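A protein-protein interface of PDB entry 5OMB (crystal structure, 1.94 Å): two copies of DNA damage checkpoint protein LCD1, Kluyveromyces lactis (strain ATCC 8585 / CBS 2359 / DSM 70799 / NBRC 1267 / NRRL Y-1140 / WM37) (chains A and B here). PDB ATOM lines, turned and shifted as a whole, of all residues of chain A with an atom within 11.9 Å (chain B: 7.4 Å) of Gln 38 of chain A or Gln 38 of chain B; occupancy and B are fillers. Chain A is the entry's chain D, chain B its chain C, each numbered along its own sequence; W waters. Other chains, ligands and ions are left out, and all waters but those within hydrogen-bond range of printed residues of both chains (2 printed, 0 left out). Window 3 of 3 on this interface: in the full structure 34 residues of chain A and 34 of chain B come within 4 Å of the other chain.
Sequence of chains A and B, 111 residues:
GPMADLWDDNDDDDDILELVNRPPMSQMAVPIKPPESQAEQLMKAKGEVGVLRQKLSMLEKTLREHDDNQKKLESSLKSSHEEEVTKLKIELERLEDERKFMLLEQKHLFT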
ATOM      1  N   PRO A  34       2.701  -9.516  21.407  1.00  0.00           N
ATOM      2  CA  PRO A  34       1.668  -9.287  20.375  1.00  0.00           C
ATOM      3  C   PRO A  34       1.110  -7.857  20.373  1.00  0.00           C
ATOM      4  O   PRO A  34       1.168  -7.193  21.420  1.00  0.00           O
ATOM      5  CB  PRO A  34       0.590 -10.327  20.706  1.00  0.00           C
ATOM      6  CG  PRO A  34       1.301 -11.385  21.444  1.00  0.00           C
ATOM      7  CD  PRO A  34       2.313 -10.640  22.285  1.00  0.00           C
ATOM      8  N   PRO A  35       0.630  -7.336  19.206  1.00  0.00           N
ATOM      9  CA  PRO A  35       0.142  -5.941  19.174  1.00  0.00           C
ATOM     10  C   PRO A  35      -0.883  -5.620  20.259  1.00  0.00           C
ATOM     11  O   PRO A  35      -1.760  -6.426  20.563  1.00  0.00           O
ATOM     12  CB  PRO A  35      -0.477  -5.795  17.780  1.00  0.00           C
ATOM     13  CG  PRO A  35       0.144  -6.852  16.960  1.00  0.00           C
ATOM     14  CD  PRO A  35       0.504  -7.985  17.883  1.00  0.00           C
ATOM     15  N   GLU A  36      -0.740  -4.452  20.863  1.00  0.00           N
ATOM     16  CA  GLU A  36      -1.692  -4.003  21.855  1.00  0.00           C
ATOM     17  C   GLU A  36      -2.405  -2.856  21.199  1.00  0.00           C
ATOM     18  O   GLU A  36      -1.775  -2.095  20.459  1.00  0.00           O
ATOM     19  CB  GLU A  36      -0.966  -3.497  23.120  1.00  0.00           C
ATOM     20  CG  GLU A  36      -0.312  -4.576  23.968  1.00  0.00           C
ATOM     21  CD  GLU A  36       0.500  -4.024  25.127  1.00  0.00           C
ATOM     22  OE1 GLU A  36       0.786  -2.803  25.144  1.00  0.00           O
ATOM     23  OE2 GLU A  36       0.878  -4.827  26.010  1.00  0.00           O
ATOM     24  N   SER A  37      -3.711  -2.708  21.448  1.00  0.00           N
ATOM     25  CA  SER A  37      -4.450  -1.571  20.875  1.00  0.00           C
ATOM     26  C   SER A  37      -3.988  -0.285  21.564  1.00  0.00           C
ATOM     27  O   SER A  37      -3.332  -0.347  22.605  1.00  0.00           O
ATOM     28  CB  SER A  37      -5.945  -1.749  21.105  1.00  0.00           C
ATOM     29  OG  SER A  37      -6.246  -1.717  22.488  1.00  0.00           O
ATOM     30  N   GLN A  38      -4.350   0.872  21.013  1.00  0.00           N
ATOM     31  CA  GLN A  38      -4.029   2.156  21.618  1.00  0.00           C
ATOM     32  C   GLN A  38      -4.617   2.251  23.040  1.00  0.00           C
ATOM     33  O   GLN A  38      -3.955   2.780  23.914  1.00  0.00           O
ATOM     34  CB  GLN A  38      -4.532   3.302  20.742  1.00  0.00           C
ATOM     35  CG  GLN A  38      -3.692   3.525  19.496  1.00  0.00           C
ATOM     36  CD  GLN A  38      -4.166   4.724  18.701  1.00  0.00           C
ATOM     37  OE1 GLN A  38      -5.361   5.065  18.656  1.00  0.00           O
ATOM     38  NE2 GLN A  38      -3.236   5.379  18.032  1.00  0.00           N
ATOM     39  N   ALA A  39      -5.828   1.698  23.282  1.00  0.00           N
ATOM     40  CA  ALA A  39      -6.454   1.705  24.613  1.00  0.00           C
ATOM     41  C   ALA A  39      -5.609   0.955  25.677  1.00  0.00           C
ATOM     42  O   ALA A  39      -5.503   1.438  26.814  1.00  0.00           O
ATOM     43  CB  ALA A  39      -7.861   1.119  24.545  1.00  0.00           C
ATOM     44  N   GLU A  40      -5.037  -0.223  25.313  1.00  0.00           N
ATOM     45  CA  GLU A  40      -4.198  -1.013  26.234  1.00  0.00           C
ATOM     46  C   GLU A  40      -2.892  -0.260  26.485  1.00  0.00           C
ATOM     47  O   GLU A  40      -2.448  -0.173  27.621  1.00  0.00           O
ATOM     48  CB  GLU A  40      -3.831  -2.404  25.653  1.00  0.00           C
ATOM     49  CG  GLU A  40      -4.991  -3.330  25.374  1.00  0.00           C
ATOM     50  CD  GLU A  40      -4.631  -4.582  24.603  1.00  0.00           C
ATOM     51  OE1 GLU A  40      -4.279  -5.594  25.250  1.00  0.00           O
ATOM     52  OE2 GLU A  40      -4.684  -4.543  23.352  1.00  0.00           O
ATOM     53  N   GLN A  41      -2.256   0.247  25.416  1.00  0.00           N
ATOM     54  CA  GLN A  41      -0.981   0.962  25.549  1.00  0.00           C
ATOM     55  C   GLN A  41      -1.131   2.230  26.354  1.00  0.00           C
ATOM     56  O   GLN A  41      -0.218   2.560  27.098  1.00  0.00           O
ATOM     57  CB  GLN A  41      -0.386   1.297  24.186  1.00  0.00           C
ATOM     58  CG  GLN A  41       0.237   0.102  23.499  1.00  0.00           C
ATOM     59  CD  GLN A  41       1.055   0.534  22.313  1.00  0.00           C
ATOM     60  OE1 GLN A  41       0.671   0.308  21.168  1.00  0.00           O
ATOM     61  NE2 GLN A  41       2.198   1.178  22.563  1.00  0.00           N
ATOM     62  N   LEU A  42      -2.271   2.946  26.200  1.00  0.00           N
ATOM     63  CA  LEU A  42      -2.519   4.190  26.940  1.00  0.00           C
ATOM     64  C   LEU A  42      -2.575   3.939  28.433  1.00  0.00           C
ATOM     65  O   LEU A  42      -1.967   4.693  29.195  1.00  0.00           O
ATOM     66  CB  LEU A  42      -3.800   4.883  26.445  1.00  0.00           C
ATOM     67  CG  LEU A  42      -4.092   6.270  27.005  1.00  0.00           C
ATOM     68  CD1 LEU A  42      -2.857   7.230  26.874  1.00  0.00           C
ATOM     69  CD2 LEU A  42      -5.330   6.848  26.346  1.00  0.00           C
ATOM     70  N   MET A  43      -3.260   2.861  28.859  1.00  0.00           N
ATOM     71  CA  MET A  43      -3.306   2.515  30.275  1.00  0.00           C
ATOM     72  C   MET A  43      -1.922   2.173  30.819  1.00  0.00           C
ATOM     73  O   MET A  43      -1.569   2.637  31.895  1.00  0.00           O
ATOM     74  CB  MET A  43      -4.293   1.381  30.552  1.00  0.00           C
ATOM     75  CG  MET A  43      -5.733   1.840  30.493  1.00  0.00           C
ATOM     76  SD  MET A  43      -6.840   0.747  31.394  1.00  0.00           S
ATOM     77  CE  MET A  43      -6.694   1.416  32.971  1.00  0.00           C
ATOM     78  N   LYS A  44      -1.120   1.417  30.063  1.00  0.00           N
ATOM     79  CA  LYS A  44       0.242   1.066  30.513  1.00  0.00           C
ATOM     80  C   LYS A  44       1.129   2.312  30.572  1.00  0.00           C
ATOM     81  O   LYS A  44       1.795   2.521  31.580  1.00  0.00           O
ATOM     82  CB  LYS A  44       0.858  -0.015  29.606  1.00  0.00           C
ATOM     83  CG  LYS A  44       0.143  -1.373  29.765  1.00  0.00           C
ATOM     84  CD  LYS A  44       0.783  -2.484  28.929  1.00  0.00           C
ATOM     85  CE  LYS A  44       0.018  -3.795  29.004  1.00  0.00           C
ATOM     86  NZ  LYS A  44      -0.060  -4.324  30.394  1.00  0.00           N
ATOM     87  N   ALA A  45       1.076   3.174  29.528  1.00  0.00           N
ATOM     88  CA  ALA A  45       1.866   4.413  29.463  1.00  0.00           C
ATOM     89  C   ALA A  45       1.483   5.390  30.576  1.00  0.00           C
ATOM     90  O   ALA A  45       2.372   5.947  31.214  1.00  0.00           O
ATOM     91  CB  ALA A  45       1.722   5.073  28.099  1.00  0.00           C
ATOM     92  N   LYS A  46       0.179   5.569  30.846  1.00  0.00           N
ATOM     93  CA  LYS A  46      -0.229   6.466  31.929  1.00  0.00           C
ATOM     94  C   LYS A  46       0.166   5.858  33.282  1.00  0.00           C
ATOM     95  O   LYS A  46       0.558   6.586  34.187  1.00  0.00           O
ATOM     96  CB  LYS A  46      -1.712   6.808  31.856  1.00  0.00           C
ATOM     97  CG  LYS A  46      -2.040   7.716  30.680  1.00  0.00           C
ATOM     98  CD  LYS A  46      -3.544   8.015  30.574  1.00  0.00           C
ATOM     99  CE  LYS A  46      -4.054   9.015  31.592  1.00  0.00           C
ATOM    100  NZ  LYS A  46      -3.318  10.311  31.582  1.00  0.00           N
ATOM    101  N   GLY A  47       0.153   4.534  33.373  1.00  0.00           N
ATOM    102  CA  GLY A  47       0.628   3.832  34.563  1.00  0.00           C
ATOM    103  C   GLY A  47       2.113   4.076  34.772  1.00  0.00           C
ATOM    104  O   GLY A  47       2.546   4.399  35.882  1.00  0.00           O
ATOM    105  N   VAL A  49       3.872   6.649  33.617  1.00  0.00           N
ATOM    106  CA  VAL A  49       4.048   8.081  33.917  1.00  0.00           C
ATOM    107  C   VAL A  49       3.910   8.292  35.455  1.00  0.00           C
ATOM    108  O   VAL A  49       4.756   8.959  36.063  1.00  0.00           O
ATOM    109  CB  VAL A  49       3.104   9.026  33.096  1.00  0.00           C
ATOM    110  CG1 VAL A  49       3.108  10.452  33.660  1.00  0.00           C
ATOM    111  CG2 VAL A  49       3.481   9.045  31.617  1.00  0.00           C
ATOM    112  N   GLU B  36      -9.048  14.846  23.482  1.00  0.00           N
ATOM    113  CA  GLU B  36      -7.857  14.425  22.771  1.00  0.00           C
ATOM    114  C   GLU B  36      -8.052  13.022  22.317  1.00  0.00           C
ATOM    115  O   GLU B  36      -8.556  12.198  23.078  1.00  0.00           O
ATOM    116  CB  GLU B  36      -6.608  14.517  23.663  1.00  0.00           C
ATOM    117  CG  GLU B  36      -6.222  15.933  24.038  1.00  0.00           C
ATOM    118  CD  GLU B  36      -4.790  16.110  24.492  1.00  0.00           C
ATOM    119  OE1 GLU B  36      -4.336  15.350  25.379  1.00  0.00           O
ATOM    120  OE2 GLU B  36      -4.129  17.040  23.977  1.00  0.00           O
ATOM    121  N   SER B  37      -7.628  12.725  21.093  1.00  0.00           N
ATOM    122  CA  SER B  37      -7.709  11.365  20.573  1.00  0.00           C
ATOM    123  C   SER B  37      -6.808  10.444  21.402  1.00  0.00           C
ATOM    124  O   SER B  37      -5.870  10.917  22.062  1.00  0.00           O
ATOM    125  CB  SER B  37      -7.257  11.344  19.124  1.00  0.00           C
ATOM    126  OG  SER B  37      -5.903  11.753  19.030  1.00  0.00           O
ATOM    127  N   GLN B  38      -7.073   9.130  21.356  1.00  0.00           N
ATOM    128  CA  GLN B  38      -6.231   8.178  22.066  1.00  0.00           C
ATOM    129  C   GLN B  38      -4.807   8.268  21.540  1.00  0.00           C
ATOM    130  O   GLN B  38      -3.870   8.179  22.333  1.00  0.00           O
ATOM    131  CB  GLN B  38      -6.768   6.762  21.905  1.00  0.00           C
ATOM    132  CG  GLN B  38      -7.932   6.461  22.820  1.00  0.00           C
ATOM    133  CD  GLN B  38      -8.420   5.040  22.683  1.00  0.00           C
ATOM    134  OE1 GLN B  38      -8.129   4.322  21.712  1.00  0.00           O
ATOM    135  NE2 GLN B  38      -9.173   4.605  23.670  1.00  0.00           N
ATOM    136  N   ALA B  39      -4.653   8.557  20.216  1.00  0.00           N
ATOM    137  CA  ALA B  39      -3.369   8.721  19.538  1.00  0.00           C
ATOM    138  C   ALA B  39      -2.568   9.891  20.138  1.00  0.00           C
ATOM    139  O   ALA B  39      -1.369   9.728  20.389  1.00  0.00           O
ATOM    140  CB  ALA B  39      -3.588   8.924  18.044  1.00  0.00           C
ATOM    141  N   GLU B  40      -3.226  11.060  20.374  1.00  0.00           N
ATOM    142  CA  GLU B  40      -2.600  12.248  20.979  1.00  0.00           C
ATOM    143  C   GLU B  40      -2.202  11.938  22.421  1.00  0.00           C
ATOM    144  O   GLU B  40      -1.080  12.226  22.813  1.00  0.00           O
ATOM    145  CB  GLU B  40      -3.565  13.444  21.013  1.00  0.00           C
ATOM    146  CG  GLU B  40      -3.864  14.096  19.675  1.00  0.00           C
ATOM    147  CD  GLU B  40      -5.062  15.021  19.702  1.00  0.00           C
ATOM    148  OE1 GLU B  40      -6.190  14.543  19.447  1.00  0.00           O
ATOM    149  OE2 GLU B  40      -4.878  16.216  20.022  1.00  0.00           O
ATOM    150  N   GLN B  41      -3.123  11.332  23.201  1.00  0.00           N
ATOM    151  CA  GLN B  41      -2.905  10.990  24.605  1.00  0.00           C
ATOM    152  C   GLN B  41      -1.743  10.010  24.793  1.00  0.00           C
ATOM    153  O   GLN B  41      -0.897  10.208  25.672  1.00  0.00           O
ATOM    154  CB  GLN B  41      -4.199  10.421  25.219  1.00  0.00           C
ATOM    155  CG  GLN B  41      -5.327  11.457  25.360  1.00  0.00           C
ATOM    156  CD  GLN B  41      -6.441  10.913  26.203  1.00  0.00           C
ATOM    157  OE1 GLN B  41      -6.269  10.665  27.396  1.00  0.00           O
ATOM    158  NE2 GLN B  41      -7.599  10.668  25.594  1.00  0.00           N
ATOM    159  N   LEU B  42      -1.659   9.010  23.921  1.00  0.00           N
ATOM    160  CA  LEU B  42      -0.633   7.963  23.991  1.00  0.00           C
ATOM    161  C   LEU B  42       0.718   8.557  23.648  1.00  0.00           C
ATOM    162  O   LEU B  42       1.692   8.316  24.356  1.00  0.00           O
ATOM    163  CB  LEU B  42      -0.995   6.798  23.017  1.00  0.00           C
ATOM    164  CG  LEU B  42      -0.087   5.557  23.021  1.00  0.00           C
ATOM    165  CD1 LEU B  42       0.241   5.066  24.444  1.00  0.00           C
ATOM    166  CD2 LEU B  42      -0.692   4.446  22.181  1.00  0.00           C
ATOM    167  N   MET B  43       0.755   9.374  22.595  1.00  0.00           N
ATOM    168  CA  MET B  43       1.999  10.033  22.199  1.00  0.00           C
ATOM    169  C   MET B  43       2.528  10.983  23.310  1.00  0.00           C
ATOM    170  O   MET B  43       3.728  11.011  23.575  1.00  0.00           O
ATOM    171  CB  MET B  43       1.773  10.791  20.879  1.00  0.00           C
ATOM    172  CG  MET B  43       2.990  11.523  20.431  1.00  0.00           C
ATOM    173  SD  MET B  43       2.968  11.973  18.703  1.00  0.00           S
ATOM    174  CE  MET B  43       1.438  12.931  18.643  1.00  0.00           C
ATOM    175  N   LYS B  44       1.633  11.773  23.918  1.00  0.00           N
ATOM    176  CA  LYS B  44       1.969  12.679  25.009  1.00  0.00           C
ATOM    177  C   LYS B  44       2.499  11.891  26.217  1.00  0.00           C
ATOM    178  O   LYS B  44       3.482  12.305  26.841  1.00  0.00           O
ATOM    179  CB  LYS B  44       0.735  13.533  25.392  1.00  0.00           C
ATOM    180  CG  LYS B  44       0.505  14.714  24.458  1.00  0.00           C
ATOM    181  CD  LYS B  44      -0.697  15.590  24.822  1.00  0.00           C
ATOM    182  CE  LYS B  44      -0.792  16.781  23.893  1.00  0.00           C
ATOM    183  NZ  LYS B  44      -1.516  17.921  24.515  1.00  0.00           N
HETATM  184  O   HOH W   1      -4.222  11.258  29.055  1.00  0.00           O
HETATM  185  O   HOH W   2      -6.791   7.777  18.071  1.00  0.00           O
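NE2 of Gln 41 of chain B is in hydrogen-bond range of O of Glu 36 of chain B, at 3.1 Å.
Among the printed residues, merely in contact across the chains: Gln 38 of chain A with Gln 38 of chain B, Gln 38 of chain A with Ala 39 of chain B, Ala 39 of chain A with Gln 38 of chain B, Gln 41 of chain A with Leu 42 of chain B, Leu 42 of chain A with Gln 41 of chain B, Leu 42 of chain A with Leu 42 of chain B and Ala 45 of chain A with Leu 42 of chain B.
Gln 38 of chain B touches just these residues of chain A: Gln 38 and Ala 39.
No residue of chain A comes within 4 Å of Ser 37 of chain B.
No residue of chain A comes within 4 Å of Glu 40 of chain B.
Leu 42 of chain B touches just these residues of chain A: Gln 41, Leu 42 and Ala 45.
Printed residues of chain B within 4 Å of Ala 39 of chain A: Gln 38 (3.8 Å).
Of the printed residues of chain B, Ala 45 of chain A touches Leu 42 (3.9 Å).
Of the printed residues of chain B, Leu 42 of chain A touches Gln 41 (3.6 Å) and Leu 42 (3.7 Å).
Printed residues of chain B within 4 Å of Gln 41 of chain A: Leu 42 (3.7 Å).
Lys 46 of chain A touches none of the printed residues of chain B.
The nearest residue of chain B that does not touch Gln 38 of chain A is Leu 42 of chain B (4.1 Å).
The nearest residue of chain A that does not touch Gln 38 of chain B is Leu 42 of chain A (4.4 Å).
The nearest printed residue of chain B that does not touch Leu 42 of chain A is Gln 38 of chain B (4.4 Å).
Printed residues of chain A that touch a printed residue of chain B: Gln 38, Ala 39, Gln 41, Leu 42 and Ala 45.
Hydrophobic or aromatic side chains of chain A within 4 Å of the printed part of chain B: Ala 39, Leu 42 and Ala 45.
Along chain A the printed residues that touch a printed residue of chain B span positions 38 to 45.
Of the 9 printed residues of chain B, 4 touch a printed residue of chain A.
Printed residues of chain B that touch a printed residue of chain A: Gln 38, Ala 39, Gln 41 and Leu 42.
Hydrophobic or aromatic side chains of chain B within 4 Å of the printed part of chain A: Ala 39 and Leu 42.
Among the printed residues, 7 pairs touch across the chains.
Among the printed residues, no Asp or Glu carboxylate lies within 4 Å of a Lys or Arg side-chain nitrogen of the other chain.
Gln 38 of chain A touches its own counterpart, Gln 38 of chain B.
Gln 38 of chain A touches Ala 39 of chain B, and with the chains exchanged Ala 39 of chain A touches Gln 38 of chain B.
Gln 41 of chain A touches Leu 42 of chain B, and with the chains exchanged Leu 42 of chain A touches Gln 41 of chain B.
Leu 42 of chain A touches its own counterpart, Leu 42 of chain B.
Of the 7 pairs that touch across the chains among the printed residues, 6 have their exchanged pair printed and touching as well.
Water W1 bridges OE1 of Gln 41 of chain B (2.7 Å) and NZ of Lys 46 of chain A (2.8 Å).
Water W2 lies within hydrogen-bond range of the side-chain amide oxygen (OE1) of Gln 38 of chain A (3.1 Å) and the backbone NH (N) of Ala 39 of chain B (3.1 Å).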
